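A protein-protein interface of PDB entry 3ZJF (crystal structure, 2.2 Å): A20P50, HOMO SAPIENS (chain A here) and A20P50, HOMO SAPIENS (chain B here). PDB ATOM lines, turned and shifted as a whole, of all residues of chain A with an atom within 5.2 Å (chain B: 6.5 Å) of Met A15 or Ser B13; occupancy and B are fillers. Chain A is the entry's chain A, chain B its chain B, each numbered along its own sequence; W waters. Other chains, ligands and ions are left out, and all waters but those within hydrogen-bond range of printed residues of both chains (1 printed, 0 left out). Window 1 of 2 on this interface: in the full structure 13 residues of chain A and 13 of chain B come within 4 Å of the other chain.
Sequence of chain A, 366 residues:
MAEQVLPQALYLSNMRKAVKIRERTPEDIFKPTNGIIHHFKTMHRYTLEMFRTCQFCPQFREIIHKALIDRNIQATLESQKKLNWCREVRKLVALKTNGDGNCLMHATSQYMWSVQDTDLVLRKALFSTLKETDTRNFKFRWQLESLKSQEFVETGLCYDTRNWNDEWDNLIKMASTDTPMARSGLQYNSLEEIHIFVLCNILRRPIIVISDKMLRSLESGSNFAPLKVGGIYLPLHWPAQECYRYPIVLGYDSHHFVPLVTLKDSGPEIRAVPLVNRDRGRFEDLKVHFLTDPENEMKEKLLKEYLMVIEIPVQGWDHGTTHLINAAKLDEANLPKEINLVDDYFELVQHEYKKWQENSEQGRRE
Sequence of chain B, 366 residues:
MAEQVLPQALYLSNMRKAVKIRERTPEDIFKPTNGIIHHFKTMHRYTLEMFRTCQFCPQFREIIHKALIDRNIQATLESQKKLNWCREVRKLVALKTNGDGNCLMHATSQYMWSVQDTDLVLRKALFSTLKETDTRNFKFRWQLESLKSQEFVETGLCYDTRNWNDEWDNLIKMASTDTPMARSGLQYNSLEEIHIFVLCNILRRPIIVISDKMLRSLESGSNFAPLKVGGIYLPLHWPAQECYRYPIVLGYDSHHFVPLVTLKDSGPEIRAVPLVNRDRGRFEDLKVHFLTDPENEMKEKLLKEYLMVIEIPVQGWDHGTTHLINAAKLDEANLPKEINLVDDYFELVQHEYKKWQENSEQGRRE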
ATOM      1  N   TYR A  11      30.895   1.660 -23.262  1.00  0.00           N
ATOM      2  CA  TYR A  11      30.934   0.217 -23.479  1.00  0.00           C
ATOM      3  C   TYR A  11      29.913  -0.496 -22.613  1.00  0.00           C
ATOM      4  O   TYR A  11      29.484  -1.597 -22.938  1.00  0.00           O
ATOM      5  CB  TYR A  11      32.364  -0.355 -23.261  1.00  0.00           C
ATOM      6  CG  TYR A  11      32.777  -0.590 -21.810  1.00  0.00           C
ATOM      7  CD1 TYR A  11      33.177   0.468 -20.990  1.00  0.00           C
ATOM      8  CD2 TYR A  11      32.778  -1.873 -21.263  1.00  0.00           C
ATOM      9  CE1 TYR A  11      33.555   0.261 -19.654  1.00  0.00           C
ATOM     10  CE2 TYR A  11      33.156  -2.095 -19.925  1.00  0.00           C
ATOM     11  CZ  TYR A  11      33.540  -1.021 -19.128  1.00  0.00           C
ATOM     12  OH  TYR A  11      33.912  -1.226 -17.807  1.00  0.00           O
ATOM     13  N   LEU A  12      29.513   0.142 -21.516  1.00  0.00           N
ATOM     14  CA  LEU A  12      28.612  -0.493 -20.562  1.00  0.00           C
ATOM     15  C   LEU A  12      27.203  -0.579 -21.118  1.00  0.00           C
ATOM     16  O   LEU A  12      26.362  -1.265 -20.558  1.00  0.00           O
ATOM     17  CB  LEU A  12      28.596   0.271 -19.233  1.00  0.00           C
ATOM     18  CG  LEU A  12      29.326  -0.369 -18.059  1.00  0.00           C
ATOM     19  CD1 LEU A  12      30.129  -1.582 -18.516  1.00  0.00           C
ATOM     20  CD2 LEU A  12      30.196   0.627 -17.291  1.00  0.00           C
ATOM     21  N   SER A  13      26.931   0.122 -22.211  1.00  0.00           N
ATOM     22  CA  SER A  13      25.559   0.139 -22.711  1.00  0.00           C
ATOM     23  C   SER A  13      25.176  -1.155 -23.425  1.00  0.00           C
ATOM     24  O   SER A  13      23.990  -1.457 -23.562  1.00  0.00           O
ATOM     25  CB  SER A  13      25.311   1.337 -23.628  1.00  0.00           C
ATOM     26  OG  SER A  13      25.722   1.056 -24.968  1.00  0.00           O
ATOM     27  N   ASN A  14      26.170  -1.900 -23.901  1.00  0.00           N
ATOM     28  CA  ASN A  14      25.913  -3.177 -24.581  1.00  0.00           C
ATOM     29  C   ASN A  14      27.189  -3.977 -24.692  1.00  0.00           C
ATOM     30  O   ASN A  14      27.810  -4.021 -25.772  1.00  0.00           O
ATOM     31  CB  ASN A  14      25.275  -2.979 -25.970  1.00  0.00           C
ATOM     32  CG  ASN A  14      24.567  -4.235 -26.485  1.00  0.00           C
ATOM     33  OD1 ASN A  14      24.906  -5.364 -26.117  1.00  0.00           O
ATOM     34  ND2 ASN A  14      23.585  -4.037 -27.353  1.00  0.00           N
ATOM     35  N   MET A  15      27.564  -4.618 -23.577  1.00  0.00           N
ATOM     36  CA  MET A  15      28.811  -5.370 -23.502  1.00  0.00           C
ATOM     37  C   MET A  15      28.792  -6.503 -24.507  1.00  0.00           C
ATOM     38  O   MET A  15      29.820  -6.839 -25.104  1.00  0.00           O
ATOM     39  CB  MET A  15      29.058  -5.916 -22.097  1.00  0.00           C
ATOM     40  CG  MET A  15      29.208  -4.853 -21.032  1.00  0.00           C
ATOM     41  SD  MET A  15      29.753  -5.565 -19.461  1.00  0.00           S
ATOM     42  CE  MET A  15      31.495  -5.784 -19.797  1.00  0.00           C
ATOM     43  N   ARG A  16      27.611  -7.071 -24.716  1.00  0.00           N
ATOM     44  CA  ARG A  16      27.473  -8.208 -25.624  1.00  0.00           C
ATOM     45  C   ARG A  16      27.823  -7.775 -27.043  1.00  0.00           C
ATOM     46  O   ARG A  16      28.584  -8.452 -27.726  1.00  0.00           O
ATOM     47  CB  ARG A  16      26.064  -8.818 -25.555  1.00  0.00           C
ATOM     48  CG  ARG A  16      25.780  -9.878 -26.621  1.00  0.00           C
ATOM     49  CD  ARG A  16      26.846 -10.958 -26.599  1.00  0.00           C
ATOM     50  NE  ARG A  16      26.665 -11.970 -27.635  1.00  0.00           N
ATOM     51  CZ  ARG A  16      27.362 -12.035 -28.764  1.00  0.00           C
ATOM     52  NH1 ARG A  16      28.317 -11.138 -29.033  1.00  0.00           N
ATOM     53  NH2 ARG A  16      27.110 -13.006 -29.623  1.00  0.00           N
ATOM     54  N   LYS A  17      27.272  -6.639 -27.462  1.00  0.00           N
ATOM     55  CA  LYS A  17      27.527  -6.093 -28.799  1.00  0.00           C
ATOM     56  C   LYS A  17      28.981  -5.653 -28.924  1.00  0.00           C
ATOM     57  O   LYS A  17      29.585  -5.791 -29.982  1.00  0.00           O
ATOM     58  CB  LYS A  17      26.549  -4.951 -29.119  1.00  0.00           C
ATOM     59  CG  LYS A  17      26.776  -4.249 -30.464  1.00  0.00           C
ATOM     60  CD  LYS A  17      25.808  -3.075 -30.698  1.00  0.00           C
ATOM     61  CE  LYS A  17      24.373  -3.569 -30.950  1.00  0.00           C
ATOM     62  NZ  LYS A  17      23.436  -2.453 -31.290  1.00  0.00           N
ATOM     63  N   ALA A  18      29.561  -5.157 -27.837  1.00  0.00           N
ATOM     64  CA  ALA A  18      30.963  -4.759 -27.872  1.00  0.00           C
ATOM     65  C   ALA A  18      31.846  -5.921 -28.300  1.00  0.00           C
ATOM     66  O   ALA A  18      32.686  -5.785 -29.190  1.00  0.00           O
ATOM     67  CB  ALA A  18      31.393  -4.232 -26.530  1.00  0.00           C
ATOM     68  N   VAL A  19      31.637  -7.062 -27.648  1.00  0.00           N
ATOM     69  CA  VAL A  19      32.353  -8.282 -27.942  1.00  0.00           C
ATOM     70  C   VAL A  19      32.088  -8.795 -29.371  1.00  0.00           C
ATOM     71  O   VAL A  19      33.004  -9.280 -30.013  1.00  0.00           O
ATOM     72  CB  VAL A  19      32.035  -9.410 -26.853  1.00  0.00           C
ATOM     73  CG1 VAL A  19      32.164 -10.814 -27.443  1.00  0.00           C
ATOM     74  CG2 VAL A  19      32.914  -9.237 -25.615  1.00  0.00           C
ATOM     75  N   LEU B   6      34.764  -9.302 -16.776  1.00  0.00           N
ATOM     76  CA  LEU B   6      33.371  -9.786 -16.813  1.00  0.00           C
ATOM     77  C   LEU B   6      32.432  -8.894 -15.976  1.00  0.00           C
ATOM     78  O   LEU B   6      32.860  -8.331 -14.966  1.00  0.00           O
ATOM     79  CB  LEU B   6      33.271 -11.276 -16.412  1.00  0.00           C
ATOM     80  N   PRO B   7      31.158  -8.746 -16.407  1.00  0.00           N
ATOM     81  CA  PRO B   7      30.167  -7.861 -15.765  1.00  0.00           C
ATOM     82  C   PRO B   7      29.937  -8.093 -14.264  1.00  0.00           C
ATOM     83  O   PRO B   7      29.811  -9.229 -13.796  1.00  0.00           O
ATOM     84  CB  PRO B   7      28.874  -8.156 -16.530  1.00  0.00           C
ATOM     85  CG  PRO B   7      29.322  -8.685 -17.840  1.00  0.00           C
ATOM     86  CD  PRO B   7      30.597  -9.424 -17.589  1.00  0.00           C
ATOM     87  N   GLN B   8      29.847  -6.984 -13.535  1.00  0.00           N
ATOM     88  CA  GLN B   8      29.765  -6.992 -12.081  1.00  0.00           C
ATOM     89  C   GLN B   8      28.455  -7.613 -11.604  1.00  0.00           C
ATOM     90  O   GLN B   8      28.427  -8.349 -10.618  1.00  0.00           O
ATOM     91  CB  GLN B   8      29.918  -5.563 -11.552  1.00  0.00           C
ATOM     92  N   ALA B   9      27.380  -7.307 -12.330  1.00  0.00           N
ATOM     93  CA  ALA B   9      26.048  -7.860 -12.098  1.00  0.00           C
ATOM     94  C   ALA B   9      25.518  -8.484 -13.401  1.00  0.00           C
ATOM     95  O   ALA B   9      26.229  -8.505 -14.407  1.00  0.00           O
ATOM     96  CB  ALA B   9      25.120  -6.749 -11.633  1.00  0.00           C
ATOM     97  N   LEU B  10      24.268  -8.950 -13.395  1.00  0.00           N
ATOM     98  CA  LEU B  10      23.636  -9.543 -14.579  1.00  0.00           C
ATOM     99  C   LEU B  10      23.157  -8.519 -15.606  1.00  0.00           C
ATOM    100  O   LEU B  10      23.403  -8.691 -16.800  1.00  0.00           O
ATOM    101  CB  LEU B  10      22.449 -10.411 -14.172  1.00  0.00           C
ATOM    102  CG  LEU B  10      21.636 -11.109 -15.272  1.00  0.00           C
ATOM    103  CD1 LEU B  10      22.538 -11.950 -16.136  1.00  0.00           C
ATOM    104  CD2 LEU B  10      20.469 -11.991 -14.663  1.00  0.00           C
ATOM    105  N   TYR B  11      22.455  -7.473 -15.153  1.00  0.00           N
ATOM    106  CA  TYR B  11      21.934  -6.430 -16.057  1.00  0.00           C
ATOM    107  C   TYR B  11      23.052  -5.713 -16.855  1.00  0.00           C
ATOM    108  O   TYR B  11      22.784  -5.078 -17.870  1.00  0.00           O
ATOM    109  CB  TYR B  11      21.046  -5.404 -15.300  1.00  0.00           C
ATOM    110  CG  TYR B  11      21.818  -4.296 -14.595  1.00  0.00           C
ATOM    111  CD1 TYR B  11      22.389  -4.510 -13.343  1.00  0.00           C
ATOM    112  CD2 TYR B  11      21.999  -3.039 -15.193  1.00  0.00           C
ATOM    113  CE1 TYR B  11      23.111  -3.518 -12.697  1.00  0.00           C
ATOM    114  CE2 TYR B  11      22.720  -2.032 -14.551  1.00  0.00           C
ATOM    115  CZ  TYR B  11      23.278  -2.280 -13.301  1.00  0.00           C
ATOM    116  OH  TYR B  11      24.000  -1.311 -12.633  1.00  0.00           O
ATOM    117  N   LEU B  12      24.296  -5.806 -16.387  1.00  0.00           N
ATOM    118  CA  LEU B  12      25.399  -5.077 -17.016  1.00  0.00           C
ATOM    119  C   LEU B  12      25.830  -5.718 -18.343  1.00  0.00           C
ATOM    120  O   LEU B  12      26.446  -5.065 -19.195  1.00  0.00           O
ATOM    121  CB  LEU B  12      26.569  -4.908 -16.038  1.00  0.00           C
ATOM    122  CG  LEU B  12      26.450  -3.663 -15.141  1.00  0.00           C
ATOM    123  CD1 LEU B  12      26.925  -3.937 -13.733  1.00  0.00           C
ATOM    124  CD2 LEU B  12      27.204  -2.471 -15.722  1.00  0.00           C
ATOM    125  N   SER B  13      25.451  -6.984 -18.496  1.00  0.00           N
ATOM    126  CA  SER B  13      25.675  -7.817 -19.671  1.00  0.00           C
ATOM    127  C   SER B  13      25.100  -7.221 -20.957  1.00  0.00           C
ATOM    128  O   SER B  13      25.714  -7.306 -22.029  1.00  0.00           O
ATOM    129  CB  SER B  13      25.056  -9.202 -19.399  1.00  0.00           C
ATOM    130  OG  SER B  13      24.827  -9.926 -20.592  1.00  0.00           O
ATOM    131  N   ASN B  14      23.932  -6.607 -20.853  1.00  0.00           N
ATOM    132  CA  ASN B  14      23.317  -5.957 -21.996  1.00  0.00           C
ATOM    133  C   ASN B  14      22.286  -4.970 -21.486  1.00  0.00           C
ATOM    134  O   ASN B  14      21.095  -5.301 -21.441  1.00  0.00           O
ATOM    135  CB  ASN B  14      22.688  -6.975 -22.977  1.00  0.00           C
ATOM    136  CG  ASN B  14      22.350  -6.364 -24.352  1.00  0.00           C
ATOM    137  OD1 ASN B  14      22.185  -5.146 -24.495  1.00  0.00           O
ATOM    138  ND2 ASN B  14      22.209  -7.224 -25.356  1.00  0.00           N
ATOM    139  N   MET B  15      22.738  -3.754 -21.145  1.00  0.00           N
ATOM    140  CA  MET B  15      21.871  -2.787 -20.482  1.00  0.00           C
ATOM    141  C   MET B  15      20.737  -2.395 -21.399  1.00  0.00           C
ATOM    142  O   MET B  15      19.639  -2.098 -20.943  1.00  0.00           O
ATOM    143  CB  MET B  15      22.634  -1.546 -20.000  1.00  0.00           C
ATOM    144  CG  MET B  15      23.637  -1.772 -18.891  1.00  0.00           C
ATOM    145  SD  MET B  15      24.152  -0.175 -18.230  1.00  0.00           S
ATOM    146  CE  MET B  15      22.595   0.425 -17.571  1.00  0.00           C
ATOM    147  N   ASN B 340      16.826 -12.333 -23.412  1.00  0.00           N
ATOM    148  CA  ASN B 340      17.509 -13.091 -22.344  1.00  0.00           C
ATOM    149  C   ASN B 340      18.897 -12.566 -21.937  1.00  0.00           C
ATOM    150  O   ASN B 340      19.901 -12.872 -22.582  1.00  0.00           O
ATOM    151  CB  ASN B 340      17.593 -14.593 -22.670  1.00  0.00           C
ATOM    152  CG  ASN B 340      17.857 -15.459 -21.412  1.00  0.00           C
ATOM    153  OD1 ASN B 340      18.404 -14.978 -20.414  1.00  0.00           O
ATOM    154  ND2 ASN B 340      17.463 -16.732 -21.465  1.00  0.00           N
ATOM    155  N   LEU B 341      18.965 -11.820 -20.834  1.00  0.00           N
ATOM    156  CA  LEU B 341      20.258 -11.317 -20.377  1.00  0.00           C
ATOM    157  C   LEU B 341      21.248 -12.458 -20.078  1.00  0.00           C
ATOM    158  O   LEU B 341      22.474 -12.323 -20.292  1.00  0.00           O
ATOM    159  CB  LEU B 341      20.113 -10.373 -19.169  1.00  0.00           C
ATOM    160  CG  LEU B 341      19.446  -8.995 -19.279  1.00  0.00           C
ATOM    161  CD1 LEU B 341      19.409  -8.316 -17.902  1.00  0.00           C
ATOM    162  CD2 LEU B 341      20.150  -8.073 -20.293  1.00  0.00           C
ATOM    163  N   VAL B 342      20.721 -13.585 -19.604  1.00  0.00           N
ATOM    164  CA  VAL B 342      21.566 -14.726 -19.282  1.00  0.00           C
ATOM    165  C   VAL B 342      22.368 -15.311 -20.475  1.00  0.00           C
ATOM    166  O   VAL B 342      23.562 -15.621 -20.305  1.00  0.00           O
ATOM    167  CB  VAL B 342      20.782 -15.840 -18.457  1.00  0.00           C
ATOM    168  CG1 VAL B 342      21.545 -17.131 -18.438  1.00  0.00           C
ATOM    169  CG2 VAL B 342      20.520 -15.367 -17.020  1.00  0.00           C
ATOM    170  N   ASP B 343      21.758 -15.422 -21.671  1.00  0.00           N
ATOM    171  CA  ASP B 343      22.501 -15.891 -22.864  1.00  0.00           C
ATOM    172  C   ASP B 343      23.611 -14.890 -23.261  1.00  0.00           C
ATOM    173  O   ASP B 343      24.674 -15.281 -23.754  1.00  0.00           O
ATOM    174  CB  ASP B 343      21.581 -16.167 -24.073  1.00  0.00           C
ATOM    175  CG  ASP B 343      20.632 -17.360 -23.851  1.00  0.00           C
ATOM    176  OD1 ASP B 343      21.023 -18.384 -23.212  1.00  0.00           O
ATOM    177  OD2 ASP B 343      19.475 -17.271 -24.327  1.00  0.00           O
ATOM    178  N   ASP B 344      23.381 -13.603 -23.034  1.00  0.00           N
ATOM    179  CA  ASP B 344      24.418 -12.614 -23.381  1.00  0.00           C
ATOM    180  C   ASP B 344      25.556 -12.729 -22.392  1.00  0.00           C
ATOM    181  O   ASP B 344      26.710 -12.736 -22.785  1.00  0.00           O
ATOM    182  CB  ASP B 344      23.871 -11.185 -23.394  1.00  0.00           C
ATOM    183  CG  ASP B 344      22.885 -10.949 -24.511  1.00  0.00           C
ATOM    184  OD1 ASP B 344      23.067 -11.502 -25.611  1.00  0.00           O
ATOM    185  OD2 ASP B 344      21.908 -10.221 -24.276  1.00  0.00           O
ATOM    186  N   TYR B 345      25.222 -12.874 -21.110  1.00  0.00           N
ATOM    187  CA  TYR B 345      26.250 -13.029 -20.093  1.00  0.00           C
ATOM    188  C   TYR B 345      27.150 -14.206 -20.466  1.00  0.00           C
ATOM    189  O   TYR B 345      28.387 -14.119 -20.392  1.00  0.00           O
ATOM    190  CB  TYR B 345      25.629 -13.232 -18.712  1.00  0.00           C
ATOM    191  CG  TYR B 345      26.589 -12.928 -17.601  1.00  0.00           C
ATOM    192  CD1 TYR B 345      27.538 -13.861 -17.199  1.00  0.00           C
ATOM    193  CD2 TYR B 345      26.562 -11.707 -16.965  1.00  0.00           C
ATOM    194  CE1 TYR B 345      28.430 -13.582 -16.190  1.00  0.00           C
ATOM    195  CE2 TYR B 345      27.464 -11.410 -15.954  1.00  0.00           C
ATOM    196  CZ  TYR B 345      28.395 -12.355 -15.576  1.00  0.00           C
ATOM    197  OH  TYR B 345      29.282 -12.069 -14.572  1.00  0.00           O
ATOM    198  N   PHE B 346      26.509 -15.277 -20.928  1.00  0.00           N
ATOM    199  CA  PHE B 346      27.189 -16.516 -21.279  1.00  0.00           C
ATOM    200  C   PHE B 346      28.074 -16.342 -22.506  1.00  0.00           C
ATOM    201  O   PHE B 346      29.185 -16.871 -22.553  1.00  0.00           O
ATOM    202  CB  PHE B 346      26.166 -17.659 -21.474  1.00  0.00           C
ATOM    203  CG  PHE B 346      26.792 -18.992 -21.777  1.00  0.00           C
ATOM    204  CD1 PHE B 346      27.356 -19.758 -20.762  1.00  0.00           C
ATOM    205  CD2 PHE B 346      26.834 -19.473 -23.082  1.00  0.00           C
ATOM    206  CE1 PHE B 346      27.940 -20.995 -21.039  1.00  0.00           C
ATOM    207  CE2 PHE B 346      27.426 -20.702 -23.375  1.00  0.00           C
ATOM    208  CZ  PHE B 346      27.977 -21.464 -22.347  1.00  0.00           C
ATOM    209  N   LEU B 348      29.457 -13.493 -23.311  1.00  0.00           N
ATOM    210  CA  LEU B 348      30.584 -12.791 -22.712  1.00  0.00           C
ATOM    211  C   LEU B 348      31.563 -13.724 -22.018  1.00  0.00           C
ATOM    212  O   LEU B 348      32.767 -13.642 -22.210  1.00  0.00           O
ATOM    213  CB  LEU B 348      30.094 -11.728 -21.742  1.00  0.00           C
ATOM    214  CG  LEU B 348      29.379 -10.533 -22.391  1.00  0.00           C
ATOM    215  CD1 LEU B 348      28.874  -9.549 -21.349  1.00  0.00           C
ATOM    216  CD2 LEU B 348      30.287  -9.830 -23.388  1.00  0.00           C
HETATM  217  O   HOH W   1      21.586  -6.724 -28.336  1.00  0.00           O
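O of Leu A12 lies close to SD of Met B15 (3.4 Å). The backbone carbonyl oxygen (O) of Leu B12 lies close to the side-chain sulfur (SD) of Met A15, at 3.4 Å. The side-chain amide oxygen (OD1) of Asn A14 lies close to the side-chain amide oxygen (OD1) of Asn B14, 3.2 Å away. N of Arg A16 is in hydrogen-bond range of O of Ser B13.
OD2 of Asp B344 lies within hydrogen-bond range of ND2 of Asn B14 (3.2 Å). The side-chain amide oxygen (OD1) of Asn A14 lies close to the backbone NH (N) of Arg A16. The backbone carbonyl oxygen (O) of Leu B341 is in hydrogen-bond range of the side-chain hydroxyl (OG) of Ser B13, at 3.4 Å. The side-chain amide oxygen (OD1) of Asn A14 sits at hydrogen-bond distance from the backbone NH (N) of Lys A17 (3.0 Å). The side-chain hydroxyl of Ser B13 lies within hydrogen-bond range of the backbone NH of Tyr B345 (3.0 Å). O of Pro B7 lies within hydrogen-bond range of OH of Tyr B345, at 3.0 Å.
CG of Leu A12 touches CD2 of Leu B12, 3.8 Å away. Ser A13 touches Met B15 (O to N, 3.6 Å). Met A15 touches Pro B7. Met A15 touches Ser B13 (N to O, 3.6 Å). Met A15 touches Leu B348 (O to CD2, 3.5 Å). Asp B344 touches Arg A16 (OD1 to CG, 3.3 Å). Leu B348 touches Arg A16 (CD2 to CA, 3.9 Å). Leu B348 touches Val A19.
Printed residues of chain B within 4 Å of Leu A12: Leu B12 (3.8 Å) and Met B15 (3.2 Å). Of the printed residues of chain B, Asn A14 touches Asn B14 (3.2 Å). Met A15 touches just these residues of chain B: Pro B7 (3.5 Å), Leu B12 (3.3 Å), Ser B13 (3.6 Å) and Leu B348 (3.5 Å). Of chain A, only Met A15 (3.6 Å) and Arg A16 (3.3 Å) come within 4 Å of Ser B13. Of the printed residues of chain A, Asn B14 touches Asn A14 (3.2 Å). The nearest residue of chain A that does not touch Ser B13 is Asn A14 (4.5 Å).
Hydrophobic or aromatic side chains of chain B that line the printed part of chain A: Pro B7, Leu B12, Met B15 and Leu B348. Of the 9 printed residues of chain A, 6 touch a printed residue of chain B. Hydrophobic or aromatic side chains of chain A that line the printed part of chain B: Leu A12, Met A15 and Val A19. Among the printed residues, 12 pairs touch across the chains.
Water W1 bridges ND2 of Asn B14 (3.1 Å) and ND2 of Asn A14 (3.5 Å).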
